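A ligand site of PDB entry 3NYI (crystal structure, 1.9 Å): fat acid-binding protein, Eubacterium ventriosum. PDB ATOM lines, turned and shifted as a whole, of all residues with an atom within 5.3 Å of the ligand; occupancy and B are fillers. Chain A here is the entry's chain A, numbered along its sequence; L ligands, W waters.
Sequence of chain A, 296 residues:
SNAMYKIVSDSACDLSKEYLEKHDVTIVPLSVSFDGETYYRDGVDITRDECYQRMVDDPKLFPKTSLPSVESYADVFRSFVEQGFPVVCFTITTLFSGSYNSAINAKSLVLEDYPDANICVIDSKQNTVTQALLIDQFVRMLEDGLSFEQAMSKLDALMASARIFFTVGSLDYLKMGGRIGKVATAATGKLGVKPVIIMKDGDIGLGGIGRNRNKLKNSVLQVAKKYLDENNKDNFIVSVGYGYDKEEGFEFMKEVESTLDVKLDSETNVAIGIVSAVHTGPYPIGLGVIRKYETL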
ATOM      1  N   LEU A  30      -7.607   1.757  20.036  1.00  0.00           N
ATOM      2  CA  LEU A  30      -8.393   1.058  21.051  1.00  0.00           C
ATOM      3  C   LEU A  30      -7.935   1.553  22.421  1.00  0.00           C
ATOM      4  O   LEU A  30      -6.971   2.317  22.506  1.00  0.00           O
ATOM      5  CB  LEU A  30      -8.245  -0.463  20.917  1.00  0.00           C
ATOM      6  CG  LEU A  30      -9.205  -1.046  19.868  1.00  0.00           C
ATOM      7  CD1 LEU A  30      -8.690  -0.859  18.417  1.00  0.00           C
ATOM      8  CD2 LEU A  30      -9.499  -2.528  20.136  1.00  0.00           C
ATOM      9  N   THR A  65      -9.474  -4.631  27.315  1.00  0.00           N
ATOM     10  CA  THR A  65      -9.423  -3.774  26.140  1.00  0.00           C
ATOM     11  C   THR A  65     -10.816  -3.250  25.883  1.00  0.00           C
ATOM     12  O   THR A  65     -11.805  -3.822  26.349  1.00  0.00           O
ATOM     13  CB  THR A  65      -8.990  -4.543  24.870  1.00  0.00           C
ATOM     14  OG1 THR A  65      -9.789  -5.722  24.742  1.00  0.00           O
ATOM     15  CG2 THR A  65      -7.535  -4.944  24.949  1.00  0.00           C
ATOM     16  N   SER A  66     -10.893  -2.190  25.103  1.00  0.00           N
ATOM     17  CA  SER A  66     -12.168  -1.665  24.680  1.00  0.00           C
ATOM     18  C   SER A  66     -12.044  -1.181  23.246  1.00  0.00           C
ATOM     19  O   SER A  66     -11.041  -0.564  22.881  1.00  0.00           O
ATOM     20  CB  SER A  66     -12.576  -0.517  25.620  1.00  0.00           C
ATOM     21  OG  SER A  66     -13.853  -0.031  25.287  1.00  0.00           O
ATOM     22  N   LEU A  67     -13.046  -1.500  22.434  1.00  0.00           N
ATOM     23  CA  LEU A  67     -13.119  -1.059  21.038  1.00  0.00           C
ATOM     24  C   LEU A  67     -13.122   0.469  20.934  1.00  0.00           C
ATOM     25  O   LEU A  67     -13.494   1.150  21.903  1.00  0.00           O
ATOM     26  CB  LEU A  67     -14.399  -1.643  20.408  1.00  0.00           C
ATOM     27  CG  LEU A  67     -15.721  -0.977  20.828  1.00  0.00           C
ATOM     28  CD1 LEU A  67     -16.872  -1.552  20.021  1.00  0.00           C
ATOM     29  CD2 LEU A  67     -16.002  -1.095  22.330  1.00  0.00           C
ATOM     30  N   ILE A  92      -9.501  -4.550  12.955  1.00  0.00           N
ATOM     31  CA  ILE A  92      -9.232  -5.911  13.411  1.00  0.00           C
ATOM     32  C   ILE A  92     -10.430  -6.806  13.019  1.00  0.00           C
ATOM     33  O   ILE A  92     -11.557  -6.305  12.846  1.00  0.00           O
ATOM     34  CB  ILE A  92      -9.023  -5.897  14.947  1.00  0.00           C
ATOM     35  CG1 ILE A  92      -8.431  -7.232  15.452  1.00  0.00           C
ATOM     36  CG2 ILE A  92     -10.361  -5.565  15.677  1.00  0.00           C
ATOM     37  CD1 ILE A  92      -8.057  -7.212  16.970  1.00  0.00           C
ATOM     38  N   PHE A  96     -12.998 -10.852  16.713  1.00  0.00           N
ATOM     39  CA  PHE A  96     -12.320 -10.514  17.976  1.00  0.00           C
ATOM     40  C   PHE A  96     -12.923  -9.271  18.648  1.00  0.00           C
ATOM     41  O   PHE A  96     -12.762  -9.084  19.844  1.00  0.00           O
ATOM     42  CB  PHE A  96     -10.826 -10.212  17.800  1.00  0.00           C
ATOM     43  CG  PHE A  96      -9.981 -11.407  17.403  1.00  0.00           C
ATOM     44  CD1 PHE A  96     -10.491 -12.692  17.456  1.00  0.00           C
ATOM     45  CD2 PHE A  96      -8.648 -11.223  17.026  1.00  0.00           C
ATOM     46  CE1 PHE A  96      -9.694 -13.792  17.089  1.00  0.00           C
ATOM     47  CE2 PHE A  96      -7.860 -12.302  16.666  1.00  0.00           C
ATOM     48  CZ  PHE A  96      -8.383 -13.581  16.702  1.00  0.00           C
ATOM     49  N   SER A  97     -13.521  -8.385  17.864  1.00  0.00           N
ATOM     50  CA  SER A  97     -13.820  -7.053  18.387  1.00  0.00           C
ATOM     51  C   SER A  97     -14.968  -6.415  17.631  1.00  0.00           C
ATOM     52  O   SER A  97     -15.167  -6.693  16.454  1.00  0.00           O
ATOM     53  CB  SER A  97     -12.584  -6.151  18.254  1.00  0.00           C
ATOM     54  OG  SER A  97     -12.866  -4.823  18.617  1.00  0.00           O
ATOM     55  N   GLY A  98     -15.700  -5.535  18.305  1.00  0.00           N
ATOM     56  CA  GLY A  98     -16.717  -4.764  17.624  1.00  0.00           C
ATOM     57  C   GLY A  98     -16.173  -3.495  16.974  1.00  0.00           C
ATOM     58  O   GLY A  98     -16.938  -2.632  16.546  1.00  0.00           O
ATOM     59  N   SER A  99     -14.846  -3.398  16.865  1.00  0.00           N
ATOM     60  CA  SER A  99     -14.205  -2.254  16.210  1.00  0.00           C
ATOM     61  C   SER A  99     -14.794  -1.963  14.815  1.00  0.00           C
ATOM     62  O   SER A  99     -15.118  -0.820  14.497  1.00  0.00           O
ATOM     63  CB  SER A  99     -12.693  -2.476  16.131  1.00  0.00           C
ATOM     64  OG  SER A  99     -12.054  -1.392  15.480  1.00  0.00           O
ATOM     65  N   ASN A 127      -5.233  -9.440  12.392  1.00  0.00           N
ATOM     66  CA  ASN A 127      -4.865  -8.745  13.623  1.00  0.00           C
ATOM     67  C   ASN A 127      -3.363  -8.547  13.560  1.00  0.00           C
ATOM     68  O   ASN A 127      -2.662  -9.261  12.819  1.00  0.00           O
ATOM     69  CB  ASN A 127      -5.232  -9.601  14.838  1.00  0.00           C
ATOM     70  CG  ASN A 127      -4.939  -8.916  16.157  1.00  0.00           C
ATOM     71  OD1 ASN A 127      -4.807  -7.684  16.242  1.00  0.00           O
ATOM     72  ND2 ASN A 127      -4.802  -9.719  17.225  1.00  0.00           N
ATOM     73  N   THR A 128      -2.868  -7.579  14.334  1.00  0.00           N
ATOM     74  CA  THR A 128      -1.434  -7.341  14.466  1.00  0.00           C
ATOM     75  C   THR A 128      -0.679  -7.585  13.133  1.00  0.00           C
ATOM     76  O   THR A 128      -1.007  -6.943  12.125  1.00  0.00           O
ATOM     77  CB  THR A 128      -0.824  -8.086  15.730  1.00  0.00           C
ATOM     78  OG1 THR A 128       0.586  -7.815  15.845  1.00  0.00           O
ATOM     79  CG2 THR A 128      -1.089  -9.617  15.716  1.00  0.00           C
ATOM     80  N   VAL A 129       0.322  -8.478  13.135  1.00  0.00           N
ATOM     81  CA  VAL A 129       1.200  -8.617  11.953  1.00  0.00           C
ATOM     82  C   VAL A 129       0.442  -8.788  10.602  1.00  0.00           C
ATOM     83  O   VAL A 129       0.847  -8.200   9.596  1.00  0.00           O
ATOM     84  CB  VAL A 129       2.305  -9.717  12.148  1.00  0.00           C
ATOM     85  CG1 VAL A 129       1.678 -11.114  12.247  1.00  0.00           C
ATOM     86  CG2 VAL A 129       3.378  -9.658  11.017  1.00  0.00           C
ATOM     87  N   ILE A 164      -1.167 -16.075  10.607  1.00  0.00           N
ATOM     88  CA  ILE A 164      -0.212 -15.872  11.679  1.00  0.00           C
ATOM     89  C   ILE A 164       0.097 -17.213  12.299  1.00  0.00           C
ATOM     90  O   ILE A 164      -0.817 -18.003  12.553  1.00  0.00           O
ATOM     91  CB  ILE A 164      -0.748 -14.961  12.835  1.00  0.00           C
ATOM     92  CG1 ILE A 164      -1.340 -13.658  12.302  1.00  0.00           C
ATOM     93  CG2 ILE A 164       0.398 -14.659  13.822  1.00  0.00           C
ATOM     94  CD1 ILE A 164      -1.911 -12.726  13.421  1.00  0.00           C
ATOM     95  N   PHE A 165       1.369 -17.472  12.538  1.00  0.00           N
ATOM     96  CA  PHE A 165       1.807 -18.664  13.234  1.00  0.00           C
ATOM     97  C   PHE A 165       2.546 -18.203  14.482  1.00  0.00           C
ATOM     98  O   PHE A 165       3.520 -17.472  14.386  1.00  0.00           O
ATOM     99  CB  PHE A 165       2.763 -19.461  12.341  1.00  0.00           C
ATOM    100  CG  PHE A 165       2.162 -19.869  11.031  1.00  0.00           C
ATOM    101  CD1 PHE A 165       1.253 -20.927  10.978  1.00  0.00           C
ATOM    102  CD2 PHE A 165       2.450 -19.178   9.858  1.00  0.00           C
ATOM    103  CE1 PHE A 165       0.666 -21.301   9.759  1.00  0.00           C
ATOM    104  CE2 PHE A 165       1.873 -19.551   8.650  1.00  0.00           C
ATOM    105  CZ  PHE A 165       0.976 -20.615   8.614  1.00  0.00           C
ATOM    106  N   PHE A 166       2.077 -18.607  15.653  1.00  0.00           N
ATOM    107  CA  PHE A 166       2.648 -18.035  16.866  1.00  0.00           C
ATOM    108  C   PHE A 166       2.461 -18.886  18.099  1.00  0.00           C
ATOM    109  O   PHE A 166       1.733 -19.887  18.078  1.00  0.00           O
ATOM    110  CB  PHE A 166       2.111 -16.620  17.114  1.00  0.00           C
ATOM    111  CG  PHE A 166       0.644 -16.543  17.475  1.00  0.00           C
ATOM    112  CD1 PHE A 166       0.248 -16.211  18.772  1.00  0.00           C
ATOM    113  CD2 PHE A 166      -0.346 -16.745  16.512  1.00  0.00           C
ATOM    114  CE1 PHE A 166      -1.103 -16.096  19.122  1.00  0.00           C
ATOM    115  CE2 PHE A 166      -1.704 -16.647  16.850  1.00  0.00           C
ATOM    116  CZ  PHE A 166      -2.084 -16.309  18.160  1.00  0.00           C
ATOM    117  N   LEU A 174      -5.713 -15.434  27.193  1.00  0.00           N
ATOM    118  CA  LEU A 174      -6.668 -15.798  26.149  1.00  0.00           C
ATOM    119  C   LEU A 174      -8.009 -16.194  26.745  1.00  0.00           C
ATOM    120  O   LEU A 174      -9.050 -15.760  26.266  1.00  0.00           O
ATOM    121  CB  LEU A 174      -6.139 -16.932  25.270  1.00  0.00           C
ATOM    122  CG  LEU A 174      -5.013 -16.570  24.306  1.00  0.00           C
ATOM    123  CD1 LEU A 174      -4.363 -17.810  23.686  1.00  0.00           C
ATOM    124  CD2 LEU A 174      -5.548 -15.625  23.221  1.00  0.00           C
ATOM    125  N   ARG A 179     -11.436 -14.594  24.017  1.00  0.00           N
ATOM    126  CA  ARG A 179     -11.226 -14.872  22.590  1.00  0.00           C
ATOM    127  C   ARG A 179     -10.507 -16.189  22.315  1.00  0.00           C
ATOM    128  O   ARG A 179     -10.093 -16.453  21.191  1.00  0.00           O
ATOM    129  CB  ARG A 179     -10.486 -13.719  21.891  1.00  0.00           C
ATOM    130  CG  ARG A 179     -11.369 -12.533  21.507  1.00  0.00           C
ATOM    131  CD  ARG A 179     -11.660 -11.600  22.726  1.00  0.00           C
ATOM    132  NE  ARG A 179     -12.438 -10.449  22.286  1.00  0.00           N
ATOM    133  CZ  ARG A 179     -13.079  -9.621  23.099  1.00  0.00           C
ATOM    134  NH1 ARG A 179     -13.020  -9.804  24.418  1.00  0.00           N
ATOM    135  NH2 ARG A 179     -13.772  -8.603  22.598  1.00  0.00           N
ATOM    136  N   MET A 199      -3.647 -18.212  13.095  1.00  0.00           N
ATOM    137  CA  MET A 199      -4.752 -17.326  12.748  1.00  0.00           C
ATOM    138  C   MET A 199      -5.024 -17.420  11.264  1.00  0.00           C
ATOM    139  O   MET A 199      -4.136 -17.194  10.439  1.00  0.00           O
ATOM    140  CB  MET A 199      -4.480 -15.878  13.125  1.00  0.00           C
ATOM    141  CG  MET A 199      -5.658 -14.981  12.787  1.00  0.00           C
ATOM    142  SD  MET A 199      -5.502 -13.127  13.384  1.00  0.00           S
ATOM    143  CE  MET A 199      -7.378 -12.621  13.024  1.00  0.00           C
ATOM    144  N   ILE A 204      -8.706 -17.717  15.424  1.00  0.00           N
ATOM    145  CA  ILE A 204      -7.586 -18.582  15.823  1.00  0.00           C
ATOM    146  C   ILE A 204      -7.959 -20.052  16.010  1.00  0.00           C
ATOM    147  O   ILE A 204      -9.087 -20.374  16.398  1.00  0.00           O
ATOM    148  CB  ILE A 204      -6.860 -18.073  17.089  1.00  0.00           C
ATOM    149  CG1 ILE A 204      -7.873 -17.712  18.183  1.00  0.00           C
ATOM    150  CG2 ILE A 204      -6.023 -16.822  16.748  1.00  0.00           C
ATOM    151  CD1 ILE A 204      -7.192 -17.231  19.483  1.00  0.00           C
ATOM    152  N   VAL A 240       7.767 -10.643  11.180  1.00  0.00           N
ATOM    153  CA  VAL A 240       7.759 -11.206  12.532  1.00  0.00           C
ATOM    154  C   VAL A 240       7.121 -10.244  13.539  1.00  0.00           C
ATOM    155  O   VAL A 240       7.219  -9.024  13.396  1.00  0.00           O
ATOM    156  CB  VAL A 240       9.210 -11.570  12.996  1.00  0.00           C
ATOM    157  CG1 VAL A 240       9.282 -11.706  14.512  1.00  0.00           C
ATOM    158  CG2 VAL A 240       9.702 -12.859  12.314  1.00  0.00           C
ATOM    159  N   GLY A 241       6.450 -10.807  14.557  1.00  0.00           N
ATOM    160  CA  GLY A 241       5.959 -10.040  15.698  1.00  0.00           C
ATOM    161  C   GLY A 241       6.544 -10.569  17.002  1.00  0.00           C
ATOM    162  O   GLY A 241       6.684 -11.783  17.195  1.00  0.00           O
ATOM    163  N   ILE A 272       4.455  -6.385  18.935  1.00  0.00           N
ATOM    164  CA  ILE A 272       3.042  -6.727  19.115  1.00  0.00           C
ATOM    165  C   ILE A 272       2.445  -5.747  20.121  1.00  0.00           C
ATOM    166  O   ILE A 272       3.018  -5.502  21.196  1.00  0.00           O
ATOM    167  CB  ILE A 272       2.889  -8.162  19.559  1.00  0.00           C
ATOM    168  CG1 ILE A 272       3.409  -9.092  18.448  1.00  0.00           C
ATOM    169  CG2 ILE A 272       1.437  -8.473  19.888  1.00  0.00           C
ATOM    170  CD1 ILE A 272       3.589 -10.515  18.912  1.00  0.00           C
ATOM    171  N   VAL A 275      -3.360  -4.099  22.162  1.00  0.00           N
ATOM    172  CA  VAL A 275      -4.601  -4.813  21.829  1.00  0.00           C
ATOM    173  C   VAL A 275      -4.420  -6.354  21.896  1.00  0.00           C
ATOM    174  O   VAL A 275      -5.211  -7.061  22.513  1.00  0.00           O
ATOM    175  CB  VAL A 275      -5.143  -4.420  20.435  1.00  0.00           C
ATOM    176  CG1 VAL A 275      -6.351  -5.284  20.060  1.00  0.00           C
ATOM    177  CG2 VAL A 275      -5.498  -2.929  20.406  1.00  0.00           C
ATOM    178  N   SER A 276      -3.373  -6.868  21.260  1.00  0.00           N
ATOM    179  CA  SER A 276      -3.127  -8.303  21.309  1.00  0.00           C
ATOM    180  C   SER A 276      -2.564  -8.762  22.640  1.00  0.00           C
ATOM    181  O   SER A 276      -2.942  -9.814  23.165  1.00  0.00           O
ATOM    182  CB  SER A 276      -2.179  -8.748  20.184  1.00  0.00           C
ATOM    183  OG  SER A 276      -2.778  -8.566  18.919  1.00  0.00           O
ATOM    184  N   HIS A 279      -4.571  -9.815  25.533  1.00  0.00           N
ATOM    185  CA  HIS A 279      -5.234 -11.088  25.341  1.00  0.00           C
ATOM    186  C   HIS A 279      -4.274 -12.287  25.224  1.00  0.00           C
ATOM    187  O   HIS A 279      -4.681 -13.414  25.520  1.00  0.00           O
ATOM    188  CB  HIS A 279      -6.197 -11.015  24.137  1.00  0.00           C
ATOM    189  CG  HIS A 279      -7.355 -10.092  24.384  1.00  0.00           C
ATOM    190  ND1 HIS A 279      -8.532 -10.523  24.957  1.00  0.00           N
ATOM    191  CD2 HIS A 279      -7.472  -8.754  24.232  1.00  0.00           C
ATOM    192  CE1 HIS A 279      -9.351  -9.491  25.099  1.00  0.00           C
ATOM    193  NE2 HIS A 279      -8.732  -8.397  24.668  1.00  0.00           N
ATOM    194  N   THR A 280      -3.022 -12.044  24.832  1.00  0.00           N
ATOM    195  CA  THR A 280      -2.054 -13.144  24.739  1.00  0.00           C
ATOM    196  C   THR A 280      -1.206 -13.300  25.986  1.00  0.00           C
ATOM    197  O   THR A 280      -0.645 -14.360  26.217  1.00  0.00           O
ATOM    198  CB  THR A 280      -1.052 -12.952  23.570  1.00  0.00           C
ATOM    199  OG1 THR A 280      -0.314 -11.736  23.753  1.00  0.00           O
ATOM    200  CG2 THR A 280      -1.777 -12.925  22.237  1.00  0.00           C
ATOM    201  N   PRO A 284       3.931 -13.188  23.593  1.00  0.00           N
ATOM    202  CA  PRO A 284       3.641 -13.773  22.276  1.00  0.00           C
ATOM    203  C   PRO A 284       4.841 -13.648  21.342  1.00  0.00           C
ATOM    204  O   PRO A 284       5.609 -12.692  21.472  1.00  0.00           O
ATOM    205  CB  PRO A 284       2.504 -12.891  21.747  1.00  0.00           C
ATOM    206  CG  PRO A 284       2.656 -11.558  22.480  1.00  0.00           C
ATOM    207  CD  PRO A 284       3.590 -11.750  23.650  1.00  0.00           C
ATOM    208  N   ILE A 285       5.008 -14.591  20.421  1.00  0.00           N
ATOM    209  CA  ILE A 285       6.064 -14.473  19.428  1.00  0.00           C
ATOM    210  C   ILE A 285       5.687 -15.319  18.223  1.00  0.00           C
ATOM    211  O   ILE A 285       5.126 -16.397  18.361  1.00  0.00           O
ATOM    212  CB  ILE A 285       7.429 -14.896  19.983  1.00  0.00           C
ATOM    213  CG1 ILE A 285       8.531 -14.642  18.951  1.00  0.00           C
ATOM    214  CG2 ILE A 285       7.410 -16.348  20.459  1.00  0.00           C
ATOM    215  CD1 ILE A 285       9.935 -14.558  19.550  1.00  0.00           C
ATOM    216  N   GLY A 286       5.940 -14.809  17.034  1.00  0.00           N
ATOM    217  CA  GLY A 286       5.486 -15.529  15.855  1.00  0.00           C
ATOM    218  C   GLY A 286       5.761 -14.776  14.575  1.00  0.00           C
ATOM    219  O   GLY A 286       6.517 -13.802  14.562  1.00  0.00           O
ATOM    220  N   LEU A 287       5.151 -15.251  13.498  1.00  0.00           N
ATOM    221  CA  LEU A 287       5.352 -14.638  12.197  1.00  0.00           C
ATOM    222  C   LEU A 287       4.036 -14.611  11.454  1.00  0.00           C
ATOM    223  O   LEU A 287       3.141 -15.411  11.720  1.00  0.00           O
ATOM    224  CB  LEU A 287       6.416 -15.401  11.386  1.00  0.00           C
ATOM    225  CG  LEU A 287       6.065 -16.818  10.916  1.00  0.00           C
ATOM    226  CD1 LEU A 287       6.785 -17.148   9.620  1.00  0.00           C
ATOM    227  CD2 LEU A 287       6.421 -17.833  11.995  1.00  0.00           C
ATOM    228  N   GLY A 288       3.911 -13.629  10.559  1.00  0.00           N
ATOM    229  CA  GLY A 288       2.756 -13.515   9.691  1.00  0.00           C
ATOM    230  C   GLY A 288       3.199 -13.570   8.242  1.00  0.00           C
ATOM    231  O   GLY A 288       4.333 -13.199   7.893  1.00  0.00           O
HETATM  232  C1  LIG L   1     -11.785  -5.063  21.988  1.00  0.00           C
HETATM  233  O1  LIG L   1     -12.699  -4.853  21.260  1.00  0.00           O
HETATM  234  O2  LIG L   1     -11.942  -4.998  23.174  1.00  0.00           O
HETATM  235  C2  LIG L   1     -10.466  -5.625  21.411  1.00  0.00           C
HETATM  236  C3  LIG L   1     -10.397  -7.168  21.600  1.00  0.00           C
HETATM  237  C4  LIG L   1      -9.027  -7.702  21.111  1.00  0.00           C
HETATM  238  C5  LIG L   1      -9.025  -9.249  21.063  1.00  0.00           C
HETATM  239  C6  LIG L   1      -7.626  -9.749  20.631  1.00  0.00           C
HETATM  240  C7  LIG L   1      -7.554 -11.299  20.664  1.00  0.00           C
HETATM  241  C8  LIG L   1      -6.193 -11.747  20.072  1.00  0.00           C
HETATM  242  C9  LIG L   1      -6.044 -13.284  20.100  1.00  0.00           C
HETATM  243  C10 LIG L   1      -4.623 -13.647  19.584  1.00  0.00           C
HETATM  244  C11 LIG L   1      -4.615 -13.515  18.062  1.00  0.00           C
HETATM  245  C12 LIG L   1      -3.450 -12.690  17.471  1.00  0.00           C
HETATM  246  C13 LIG L   1      -2.203 -12.607  18.359  1.00  0.00           C
HETATM  247  C14 LIG L   1      -0.980 -12.879  17.424  1.00  0.00           C
HETATM  248  C15 LIG L   1       0.336 -12.439  18.096  1.00  0.00           C
HETATM  249  C16 LIG L   1       1.519 -13.068  17.312  1.00  0.00           C
HETATM  250  C17 LIG L   1       1.910 -12.136  16.138  1.00  0.00           C
HETATM  251  C18 LIG L   1       3.200 -12.645  15.442  1.00  0.00           C
HETATM  252  O   HOH W   1     -15.342  -5.545  21.135  1.00  0.00           O
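Residues that only touch the ligand: Asn 127 (3.3 Å), Gly 286 (3.4 Å), Leu 30 (3.5 Å), Phe 96 (3.5 Å), His 279 (3.6 Å), Ser 66 (3.6 Å), Leu 67 (3.6 Å), Phe 166 (3.6 Å), Ile 272 (3.6 Å), Thr 128 (3.7 Å), Ile 164 (3.7 Å), Val 275 (3.8 Å), Leu 287 (3.8 Å), Arg 179 (3.8 Å), Gly 241 (3.8 Å), Ile 204 (3.8 Å), Val 129 (3.9 Å), Thr 280 (3.9 Å) and Leu 174 (3.9 Å).
Within 4 Å of the ligand: Leu 30, Thr 65, Ser 66, Leu 67, Phe 96, Ser 97, Asn 127, Thr 128, Val 129, Ile 164, Phe 166, Leu 174, Arg 179, Ile 204, Gly 241, Ile 272, Val 275, His 279, Thr 280, Gly 286 and Leu 287.
The nearest printed residue that does not touch the ligand is Ser 276 (4.1 Å).
Water W1 lies within hydrogen-bond range of O1 of the ligand and N of Gly 98.
OG of Ser 97 is in hydrogen-bond range of N of Ser 99 (3.0 Å).
The side-chain hydroxyl (OG1) of Thr 65 lies within hydrogen-bond range of a ring nitrogen (NE2) of His 279.
OG of Ser 276 sits at hydrogen-bond distance from ND2 of Asn 127.
O of Gly 286 is in hydrogen-bond range of N of Gly 241.
O of His 279 sits at hydrogen-bond distance from N of Leu 174 (2.8 Å).
The backbone NH of Met 199 lies within hydrogen-bond range of the backbone carbonyl oxygen of Ile 164, 2.9 Å away.
N of Arg 179 lies within hydrogen-bond range of O of Leu 174, at 3.5 Å.
OG1 of Thr 280 is in hydrogen-bond range of O of Ser 276 (3.3 Å).
An oxygen (O1) of the ligand lies within hydrogen-bond range of the side-chain hydroxyl (OG) of Ser 97.
O2 of the ligand is in hydrogen-bond range of OG1 of Thr 65.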
